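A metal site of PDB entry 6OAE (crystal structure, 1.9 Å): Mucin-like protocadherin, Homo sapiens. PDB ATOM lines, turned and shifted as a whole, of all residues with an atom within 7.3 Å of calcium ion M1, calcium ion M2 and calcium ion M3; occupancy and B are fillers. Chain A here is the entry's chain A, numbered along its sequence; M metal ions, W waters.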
ATOM      1  N   GLU A  17     -10.063 -22.633  30.851  1.00  0.00           N
ATOM      2  CA  GLU A  17      -8.699 -22.283  31.311  1.00  0.00           C
ATOM      3  C   GLU A  17      -8.586 -20.771  31.358  1.00  0.00           C
ATOM      4  O   GLU A  17      -9.331 -20.085  30.616  1.00  0.00           O
ATOM      5  CB  GLU A  17      -7.629 -22.913  30.429  1.00  0.00           C
ATOM      6  CG  GLU A  17      -7.702 -22.496  28.969  1.00  0.00           C
ATOM      7  CD  GLU A  17      -6.437 -22.831  28.211  1.00  0.00           C
ATOM      8  OE1 GLU A  17      -6.531 -22.983  26.985  1.00  0.00           O
ATOM      9  OE2 GLU A  17      -5.382 -22.930  28.849  1.00  0.00           O
ATOM     10  N   ASN A  18      -7.707 -20.268  32.228  1.00  0.00           N
ATOM     11  CA  ASN A  18      -7.434 -18.819  32.447  1.00  0.00           C
ATOM     12  C   ASN A  18      -8.603 -18.150  33.182  1.00  0.00           C
ATOM     13  O   ASN A  18      -8.546 -16.943  33.318  1.00  0.00           O
ATOM     14  CB  ASN A  18      -7.063 -18.112  31.137  1.00  0.00           C
ATOM     15  CG  ASN A  18      -5.939 -18.841  30.426  1.00  0.00           C
ATOM     16  OD1 ASN A  18      -5.058 -19.390  31.079  1.00  0.00           O
ATOM     17  ND2 ASN A  18      -5.970 -18.850  29.106  1.00  0.00           N
ATOM     18  N   PRO A  60      -6.640 -22.442  36.089  1.00  0.00           N
ATOM     19  CA  PRO A  60      -6.219 -23.597  35.307  1.00  0.00           C
ATOM     20  C   PRO A  60      -5.599 -23.235  33.955  1.00  0.00           C
ATOM     21  O   PRO A  60      -5.886 -22.150  33.422  1.00  0.00           O
ATOM     22  CB  PRO A  60      -7.521 -24.368  35.022  1.00  0.00           C
ATOM     23  CG  PRO A  60      -8.513 -23.824  35.998  1.00  0.00           C
ATOM     24  CD  PRO A  60      -8.096 -22.404  36.264  1.00  0.00           C
ATOM     25  N   ASP A  61      -4.762 -24.137  33.452  1.00  0.00           N
ATOM     26  CA  ASP A  61      -4.088 -24.029  32.140  1.00  0.00           C
ATOM     27  C   ASP A  61      -4.223 -25.373  31.447  1.00  0.00           C
ATOM     28  O   ASP A  61      -3.550 -26.321  31.860  1.00  0.00           O
ATOM     29  CB  ASP A  61      -2.633 -23.607  32.300  1.00  0.00           C
ATOM     30  CG  ASP A  61      -1.822 -23.632  31.006  1.00  0.00           C
ATOM     31  OD1 ASP A  61      -2.424 -23.790  29.945  1.00  0.00           O
ATOM     32  OD2 ASP A  61      -0.603 -23.522  31.093  1.00  0.00           O
ATOM     33  N   TYR A  62      -5.068 -25.428  30.423  1.00  0.00           N
ATOM     34  CA  TYR A  62      -5.363 -26.649  29.634  1.00  0.00           C
ATOM     35  C   TYR A  62      -4.077 -27.301  29.096  1.00  0.00           C
ATOM     36  O   TYR A  62      -4.033 -28.558  29.012  1.00  0.00           O
ATOM     37  CB  TYR A  62      -6.322 -26.329  28.507  1.00  0.00           C
ATOM     38  CG  TYR A  62      -6.747 -27.534  27.734  1.00  0.00           C
ATOM     39  CD1 TYR A  62      -7.845 -28.280  28.123  1.00  0.00           C
ATOM     40  CD2 TYR A  62      -6.036 -27.957  26.616  1.00  0.00           C
ATOM     41  CE1 TYR A  62      -8.249 -29.416  27.422  1.00  0.00           C
ATOM     42  CE2 TYR A  62      -6.423 -29.084  25.904  1.00  0.00           C
ATOM     43  CZ  TYR A  62      -7.529 -29.817  26.318  1.00  0.00           C
ATOM     44  OH  TYR A  62      -7.903 -30.922  25.607  1.00  0.00           O
ATOM     45  N   GLU A  63      -3.054 -26.503  28.757  1.00  0.00           N
ATOM     46  CA  GLU A  63      -1.756 -27.004  28.213  1.00  0.00           C
ATOM     47  C   GLU A  63      -0.889 -27.632  29.333  1.00  0.00           C
ATOM     48  O   GLU A  63      -0.004 -28.411  29.006  1.00  0.00           O
ATOM     49  CB  GLU A  63      -1.028 -25.871  27.487  1.00  0.00           C
ATOM     50  CG  GLU A  63      -1.585 -25.560  26.097  1.00  0.00           C
ATOM     51  CD  GLU A  63      -2.951 -24.879  26.033  1.00  0.00           C
ATOM     52  OE1 GLU A  63      -3.115 -23.809  26.662  1.00  0.00           O
ATOM     53  OE2 GLU A  63      -3.843 -25.384  25.336  1.00  0.00           O
ATOM     54  N   GLU A  64      -1.127 -27.300  30.603  1.00  0.00           N
ATOM     55  CA  GLU A  64      -0.380 -27.880  31.752  1.00  0.00           C
ATOM     56  C   GLU A  64      -1.142 -29.097  32.288  1.00  0.00           C
ATOM     57  O   GLU A  64      -0.502 -30.152  32.476  1.00  0.00           O
ATOM     58  CB  GLU A  64      -0.152 -26.766  32.785  1.00  0.00           C
ATOM     59  CG  GLU A  64       0.593 -27.203  34.045  1.00  0.00           C
ATOM     60  CD  GLU A  64      -0.274 -27.503  35.254  1.00  0.00           C
ATOM     61  OE1 GLU A  64      -1.338 -26.851  35.423  1.00  0.00           O
ATOM     62  OE2 GLU A  64       0.115 -28.392  36.050  1.00  0.00           O
ATOM     63  N   LEU A  91     -11.470 -26.608  30.155  1.00  0.00           N
ATOM     64  CA  LEU A  91     -11.831 -26.443  28.727  1.00  0.00           C
ATOM     65  C   LEU A  91     -10.746 -25.621  28.042  1.00  0.00           C
ATOM     66  O   LEU A  91     -10.328 -24.571  28.594  1.00  0.00           O
ATOM     67  CB  LEU A  91     -13.186 -25.750  28.584  1.00  0.00           C
ATOM     68  CG  LEU A  91     -14.365 -26.435  29.283  1.00  0.00           C
ATOM     69  CD1 LEU A  91     -15.653 -25.664  28.995  1.00  0.00           C
ATOM     70  CD2 LEU A  91     -14.492 -27.889  28.860  1.00  0.00           C
ATOM     71  N   ASP A  92     -10.329 -26.083  26.882  1.00  0.00           N
ATOM     72  CA  ASP A  92      -9.292 -25.406  26.082  1.00  0.00           C
ATOM     73  C   ASP A  92      -9.850 -24.094  25.538  1.00  0.00           C
ATOM     74  O   ASP A  92     -11.040 -24.030  25.104  1.00  0.00           O
ATOM     75  CB  ASP A  92      -8.769 -26.303  24.956  1.00  0.00           C
ATOM     76  CG  ASP A  92      -7.679 -25.624  24.147  1.00  0.00           C
ATOM     77  OD1 ASP A  92      -6.809 -24.926  24.783  1.00  0.00           O
ATOM     78  OD2 ASP A  92      -7.719 -25.736  22.895  1.00  0.00           O
ATOM     79  N   VAL A  93      -9.012 -23.071  25.584  1.00  0.00           N
ATOM     80  CA  VAL A  93      -9.225 -21.727  24.993  1.00  0.00           C
ATOM     81  C   VAL A  93      -8.106 -21.536  23.954  1.00  0.00           C
ATOM     82  O   VAL A  93      -6.986 -22.094  24.148  1.00  0.00           O
ATOM     83  CB  VAL A  93      -9.194 -20.654  26.103  1.00  0.00           C
ATOM     84  CG1 VAL A  93      -9.029 -19.236  25.557  1.00  0.00           C
ATOM     85  CG2 VAL A  93     -10.436 -20.756  26.992  1.00  0.00           C
ATOM     86  N   ASN A  94      -8.394 -20.804  22.884  1.00  0.00           N
ATOM     87  CA  ASN A  94      -7.365 -20.422  21.884  1.00  0.00           C
ATOM     88  C   ASN A  94      -6.530 -19.302  22.528  1.00  0.00           C
ATOM     89  O   ASN A  94      -6.830 -18.115  22.282  1.00  0.00           O
ATOM     90  CB  ASN A  94      -8.002 -20.051  20.534  1.00  0.00           C
ATOM     91  CG  ASN A  94      -6.972 -19.663  19.497  1.00  0.00           C
ATOM     92  OD1 ASN A  94      -5.787 -19.871  19.732  1.00  0.00           O
ATOM     93  ND2 ASN A  94      -7.401 -19.115  18.373  1.00  0.00           N
ATOM     94  N   ASP A  95      -5.544 -19.665  23.351  1.00  0.00           N
ATOM     95  CA  ASP A  95      -4.752 -18.699  24.160  1.00  0.00           C
ATOM     96  C   ASP A  95      -3.277 -18.674  23.742  1.00  0.00           C
ATOM     97  O   ASP A  95      -2.495 -17.957  24.405  1.00  0.00           O
ATOM     98  CB  ASP A  95      -4.929 -18.962  25.666  1.00  0.00           C
ATOM     99  CG  ASP A  95      -4.448 -20.312  26.180  1.00  0.00           C
ATOM    100  OD1 ASP A  95      -4.377 -21.263  25.391  1.00  0.00           O
ATOM    101  OD2 ASP A  95      -4.149 -20.410  27.424  1.00  0.00           O
ATOM    102  N   ASN A  96      -2.899 -19.409  22.680  1.00  0.00           N
ATOM    103  CA  ASN A  96      -1.514 -19.490  22.154  1.00  0.00           C
ATOM    104  C   ASN A  96      -1.530 -19.083  20.673  1.00  0.00           C
ATOM    105  O   ASN A  96      -2.496 -19.421  19.961  1.00  0.00           O
ATOM    106  CB  ASN A  96      -0.930 -20.890  22.354  1.00  0.00           C
ATOM    107  CG  ASN A  96      -0.687 -21.187  23.824  1.00  0.00           C
ATOM    108  OD1 ASN A  96       0.346 -20.803  24.372  1.00  0.00           O
ATOM    109  ND2 ASN A  96      -1.620 -21.846  24.465  1.00  0.00           N
ATOM    110  N   ALA A  97      -0.496 -18.354  20.255  1.00  0.00           N
ATOM    111  CA  ALA A  97      -0.328 -17.909  18.846  1.00  0.00           C
ATOM    112  C   ALA A  97       0.523 -18.946  18.118  1.00  0.00           C
ATOM    113  O   ALA A  97       1.409 -19.580  18.722  1.00  0.00           O
ATOM    114  CB  ALA A  97       0.286 -16.534  18.800  1.00  0.00           C
ATOM    115  N   PRO A  98       0.279 -19.194  16.819  1.00  0.00           N
ATOM    116  CA  PRO A  98       1.165 -20.053  16.046  1.00  0.00           C
ATOM    117  C   PRO A  98       2.480 -19.294  15.866  1.00  0.00           C
ATOM    118  O   PRO A  98       2.477 -18.079  15.825  1.00  0.00           O
ATOM    119  CB  PRO A  98       0.408 -20.319  14.728  1.00  0.00           C
ATOM    120  CG  PRO A  98      -0.514 -19.109  14.593  1.00  0.00           C
ATOM    121  CD  PRO A  98      -0.846 -18.695  16.014  1.00  0.00           C
ATOM    122  N   ASP A 129       1.678 -24.401  17.210  1.00  0.00           N
ATOM    123  CA  ASP A 129       0.750 -23.690  18.113  1.00  0.00           C
ATOM    124  C   ASP A 129       0.563 -24.569  19.347  1.00  0.00           C
ATOM    125  O   ASP A 129       0.148 -25.747  19.176  1.00  0.00           O
ATOM    126  CB  ASP A 129      -0.539 -23.408  17.331  1.00  0.00           C
ATOM    127  CG  ASP A 129      -1.523 -22.539  18.056  1.00  0.00           C
ATOM    128  OD1 ASP A 129      -1.658 -22.689  19.298  1.00  0.00           O
ATOM    129  OD2 ASP A 129      -2.162 -21.720  17.372  1.00  0.00           O
ATOM    130  N   ARG A 130       0.855 -24.038  20.542  1.00  0.00           N
ATOM    131  CA  ARG A 130       0.766 -24.806  21.820  1.00  0.00           C
ATOM    132  C   ARG A 130      -0.694 -25.164  22.136  1.00  0.00           C
ATOM    133  O   ARG A 130      -0.896 -25.991  23.032  1.00  0.00           O
ATOM    134  CB  ARG A 130       1.480 -24.049  22.953  1.00  0.00           C
ATOM    135  CG  ARG A 130       2.993 -23.955  22.772  1.00  0.00           C
ATOM    136  CD  ARG A 130       3.689 -23.277  23.938  1.00  0.00           C
ATOM    137  NE  ARG A 130       5.139 -23.254  23.770  1.00  0.00           N
ATOM    138  CZ  ARG A 130       5.933 -24.309  23.901  1.00  0.00           C
ATOM    139  NH1 ARG A 130       7.241 -24.186  23.710  1.00  0.00           N
ATOM    140  NH2 ARG A 130       5.436 -25.495  24.237  1.00  0.00           N
ATOM    141  N   ASP A 131      -1.686 -24.604  21.453  1.00  0.00           N
ATOM    142  CA  ASP A 131      -3.062 -25.158  21.429  1.00  0.00           C
ATOM    143  C   ASP A 131      -2.995 -26.377  20.504  1.00  0.00           C
ATOM    144  O   ASP A 131      -3.165 -26.210  19.279  1.00  0.00           O
ATOM    145  CB  ASP A 131      -4.086 -24.132  20.970  1.00  0.00           C
ATOM    146  CG  ASP A 131      -4.118 -22.898  21.837  1.00  0.00           C
ATOM    147  OD1 ASP A 131      -4.162 -23.073  23.074  1.00  0.00           O
ATOM    148  OD2 ASP A 131      -4.084 -21.778  21.294  1.00  0.00           O
ATOM    149  N   LYS A 132      -2.743 -27.552  21.059  1.00  0.00           N
ATOM    150  CA  LYS A 132      -2.449 -28.783  20.282  1.00  0.00           C
ATOM    151  C   LYS A 132      -3.590 -29.100  19.297  1.00  0.00           C
ATOM    152  O   LYS A 132      -3.313 -29.715  18.277  1.00  0.00           O
ATOM    153  CB  LYS A 132      -2.274 -29.979  21.215  1.00  0.00           C
ATOM    154  CG  LYS A 132      -1.004 -30.004  22.055  1.00  0.00           C
ATOM    155  CD  LYS A 132      -0.652 -31.413  22.548  1.00  0.00           C
ATOM    156  CE  LYS A 132      -1.389 -31.862  23.805  1.00  0.00           C
ATOM    157  NZ  LYS A 132      -2.867 -31.730  23.745  1.00  0.00           N
ATOM    158  N   ASP A 134      -5.532 -26.923  17.639  1.00  0.00           N
ATOM    159  CA  ASP A 134      -5.749 -25.859  16.620  1.00  0.00           C
ATOM    160  C   ASP A 134      -5.269 -26.371  15.254  1.00  0.00           C
ATOM    161  O   ASP A 134      -4.120 -26.837  15.183  1.00  0.00           O
ATOM    162  CB  ASP A 134      -5.044 -24.553  17.000  1.00  0.00           C
ATOM    163  CG  ASP A 134      -5.774 -23.717  18.036  1.00  0.00           C
ATOM    164  OD1 ASP A 134      -6.844 -24.169  18.519  1.00  0.00           O
ATOM    165  OD2 ASP A 134      -5.288 -22.603  18.327  1.00  0.00           O
ATOM    166  N   LEU A 136      -4.036 -25.272  11.669  1.00  0.00           N
ATOM    167  CA  LEU A 136      -3.383 -24.035  11.184  1.00  0.00           C
ATOM    168  C   LEU A 136      -3.677 -23.864   9.692  1.00  0.00           C
ATOM    169  O   LEU A 136      -3.690 -24.853   8.959  1.00  0.00           O
ATOM    170  CB  LEU A 136      -1.883 -24.108  11.493  1.00  0.00           C
ATOM    171  CG  LEU A 136      -1.555 -24.237  12.983  1.00  0.00           C
ATOM    172  CD1 LEU A 136      -0.062 -24.077  13.216  1.00  0.00           C
ATOM    173  CD2 LEU A 136      -2.337 -23.244  13.828  1.00  0.00           C
ATOM    174  N   ARG A 182      -2.563 -18.659  10.426  1.00  0.00           N
ATOM    175  CA  ARG A 182      -3.541 -18.296  11.489  1.00  0.00           C
ATOM    176  C   ARG A 182      -4.048 -19.604  12.084  1.00  0.00           C
ATOM    177  O   ARG A 182      -3.951 -20.663  11.401  1.00  0.00           O
ATOM    178  CB  ARG A 182      -4.648 -17.383  10.955  1.00  0.00           C
ATOM    179  CG  ARG A 182      -5.511 -17.999   9.880  1.00  0.00           C
ATOM    180  CD  ARG A 182      -6.767 -17.218   9.489  1.00  0.00           C
ATOM    181  NE  ARG A 182      -7.536 -18.027   8.538  1.00  0.00           N
ATOM    182  CZ  ARG A 182      -7.341 -18.086   7.208  1.00  0.00           C
ATOM    183  NH1 ARG A 182      -6.416 -17.352   6.608  1.00  0.00           N
ATOM    184  NH2 ARG A 182      -8.102 -18.869   6.483  1.00  0.00           N
ATOM    185  N   ASP A 183      -4.583 -19.543  13.313  1.00  0.00           N
ATOM    186  CA  ASP A 183      -5.047 -20.742  14.054  1.00  0.00           C
ATOM    187  C   ASP A 183      -6.577 -20.842  14.011  1.00  0.00           C
ATOM    188  O   ASP A 183      -7.126 -21.563  14.830  1.00  0.00           O
ATOM    189  CB  ASP A 183      -4.501 -20.728  15.475  1.00  0.00           C
ATOM    190  CG  ASP A 183      -4.828 -19.483  16.294  1.00  0.00           C
ATOM    191  OD1 ASP A 183      -5.606 -18.609  15.803  1.00  0.00           O
ATOM    192  OD2 ASP A 183      -4.269 -19.402  17.404  1.00  0.00           O
ATOM    193  N   THR A 184      -7.243 -20.142  13.090  1.00  0.00           N
ATOM    194  CA  THR A 184      -8.716 -20.187  12.888  1.00  0.00           C
ATOM    195  C   THR A 184      -9.013 -20.267  11.398  1.00  0.00           C
ATOM    196  O   THR A 184      -8.283 -19.709  10.575  1.00  0.00           O
ATOM    197  CB  THR A 184      -9.403 -18.971  13.515  1.00  0.00           C
ATOM    198  OG1 THR A 184      -8.940 -17.772  12.869  1.00  0.00           O
ATOM    199  CG2 THR A 184      -9.171 -18.913  15.013  1.00  0.00           C
ATOM    200  N   SER A 192      -8.243 -14.987  17.366  1.00  0.00           N
ATOM    201  CA  SER A 192      -7.464 -15.512  16.209  1.00  0.00           C
ATOM    202  C   SER A 192      -6.041 -14.941  16.273  1.00  0.00           C
ATOM    203  O   SER A 192      -5.913 -13.750  16.510  1.00  0.00           O
ATOM    204  CB  SER A 192      -8.122 -15.187  14.902  1.00  0.00           C
ATOM    205  OG  SER A 192      -7.376 -15.734  13.827  1.00  0.00           O
ATOM    206  N   HIS A 193      -5.033 -15.762  16.055  1.00  0.00           N
ATOM    207  CA  HIS A 193      -3.622 -15.323  16.121  1.00  0.00           C
ATOM    208  C   HIS A 193      -2.971 -15.592  14.782  1.00  0.00           C
ATOM    209  O   HIS A 193      -3.240 -16.665  14.226  1.00  0.00           O
ATOM    210  CB  HIS A 193      -2.891 -16.049  17.231  1.00  0.00           C
ATOM    211  CG  HIS A 193      -3.599 -15.998  18.541  1.00  0.00           C
ATOM    212  ND1 HIS A 193      -4.304 -17.068  19.010  1.00  0.00           N
ATOM    213  CD2 HIS A 193      -3.719 -15.004  19.459  1.00  0.00           C
ATOM    214  CE1 HIS A 193      -4.831 -16.760  20.186  1.00  0.00           C
ATOM    215  NE2 HIS A 193      -4.496 -15.483  20.474  1.00  0.00           N
HETATM  216 CA    CA M   1      -3.844 -21.013  19.021  1.00  0.00          CA
HETATM  217 CA    CA M   2      -5.233 -23.366  25.074  1.00  0.00          CA
HETATM  218 CA    CA M   3      -3.207 -22.196  28.333  1.00  0.00          CA
HETATM  219  O   HOH W   1      -2.913 -20.758  30.244  1.00  0.00           O
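Four residues have an atom within 4 Å of calcium ion M3: Glu 17, Asp 61, Glu 63 and Asp 95. The nearest printed residue that does not touch calcium ion M3 is Asn 96 (4.2 Å).
Calcium ion M1 is bound by OD2 of Asp 134, 2.3 Å away. Calcium ion M1 is bound by O of Asn 96, at 2.3 Å. OD2 of Asp 183 is bound to calcium ion M1 (2.3 Å). The side-chain amide oxygen (OD1) of Asn 94 binds calcium ion M1. Calcium ion M1 is bound by the side-chain carboxylate (OD2) of Asp 131 (2.4 Å). Calcium ion M1 is bound by OD2 of Asp 129, at 2.5 Å. The side-chain carboxylate (OD1) of Asp 129 binds calcium ion M1 (2.8 Å).
Calcium ion M2 is bound by the side-chain carboxylate (OD1) of Asp 92 (2.2 Å), the side-chain carboxylate (OD1) of Asp 131 (2.3 Å), the side-chain carboxylate (OD1) of Asp 95 (2.3 Å), the side-chain carboxylate (OE1) of Glu 17 (2.3 Å), the backbone carbonyl oxygen (O) of Val 93 (2.4 Å), the side-chain carboxylate (OE2) of Glu 63 (2.5 Å) and the side-chain carboxylate (OE1) of Glu 63 (2.7 Å).
OD2 of Asp 95 binds calcium ion M3, 2.2 Å away. OE1 of Glu 63 is bound to calcium ion M3, 2.3 Å away. The side-chain carboxylate (OE2) of Glu 17 binds calcium ion M3, at 2.4 Å. Calcium ion M3 is bound by OD1 of Asp 61, 2.4 Å away. Water W1 is bound to calcium ion M3 (2.4 Å).
Residues that only touch calcium ion M1: His 193 (3.97 Å). Of the 26 residues printed, 7 come within 4 Å of calcium ion M1.
The side-chain amide nitrogen (ND2) of Asn 96 sits close to the side-chain carboxylate (OD1) of Asp 95. The side-chain carboxylate (OD2) of Asp 95 sits close to the side-chain amide nitrogen (ND2) of Asn 18, at 2.9 Å. The side-chain carboxylate (OE1) of Glu 63 sits close to the side-chain amide nitrogen (ND2) of Asn 96 (3.3 Å). ND1 of His 193 lies close to O of Asn 96 (3.1 Å). The backbone NH of His 193 is in hydrogen-bond range of the side-chain carboxylate of Asp 183, at 2.9 Å. OE2 of Glu 17 sits close to N of Tyr 62 (3.0 Å). The backbone carbonyl oxygen of Leu 91 lies within hydrogen-bond range of the backbone NH of Glu 17 (3.0 Å). A ring nitrogen (ND1) of His 193 lies close to the side-chain amide oxygen (OD1) of Asn 94 (3.3 Å).
Seven residues have an atom within 4 Å of calcium ion M2: Glu 17, Glu 63, Asp 92, Val 93, Asp 95, Asn 96 and Asp 131. Along chain A the residues within 4 Å of calcium ion M2 span positions 17 to 131. The nearest printed residue that does not touch calcium ion M2 is Asn 94 (4.6 Å).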
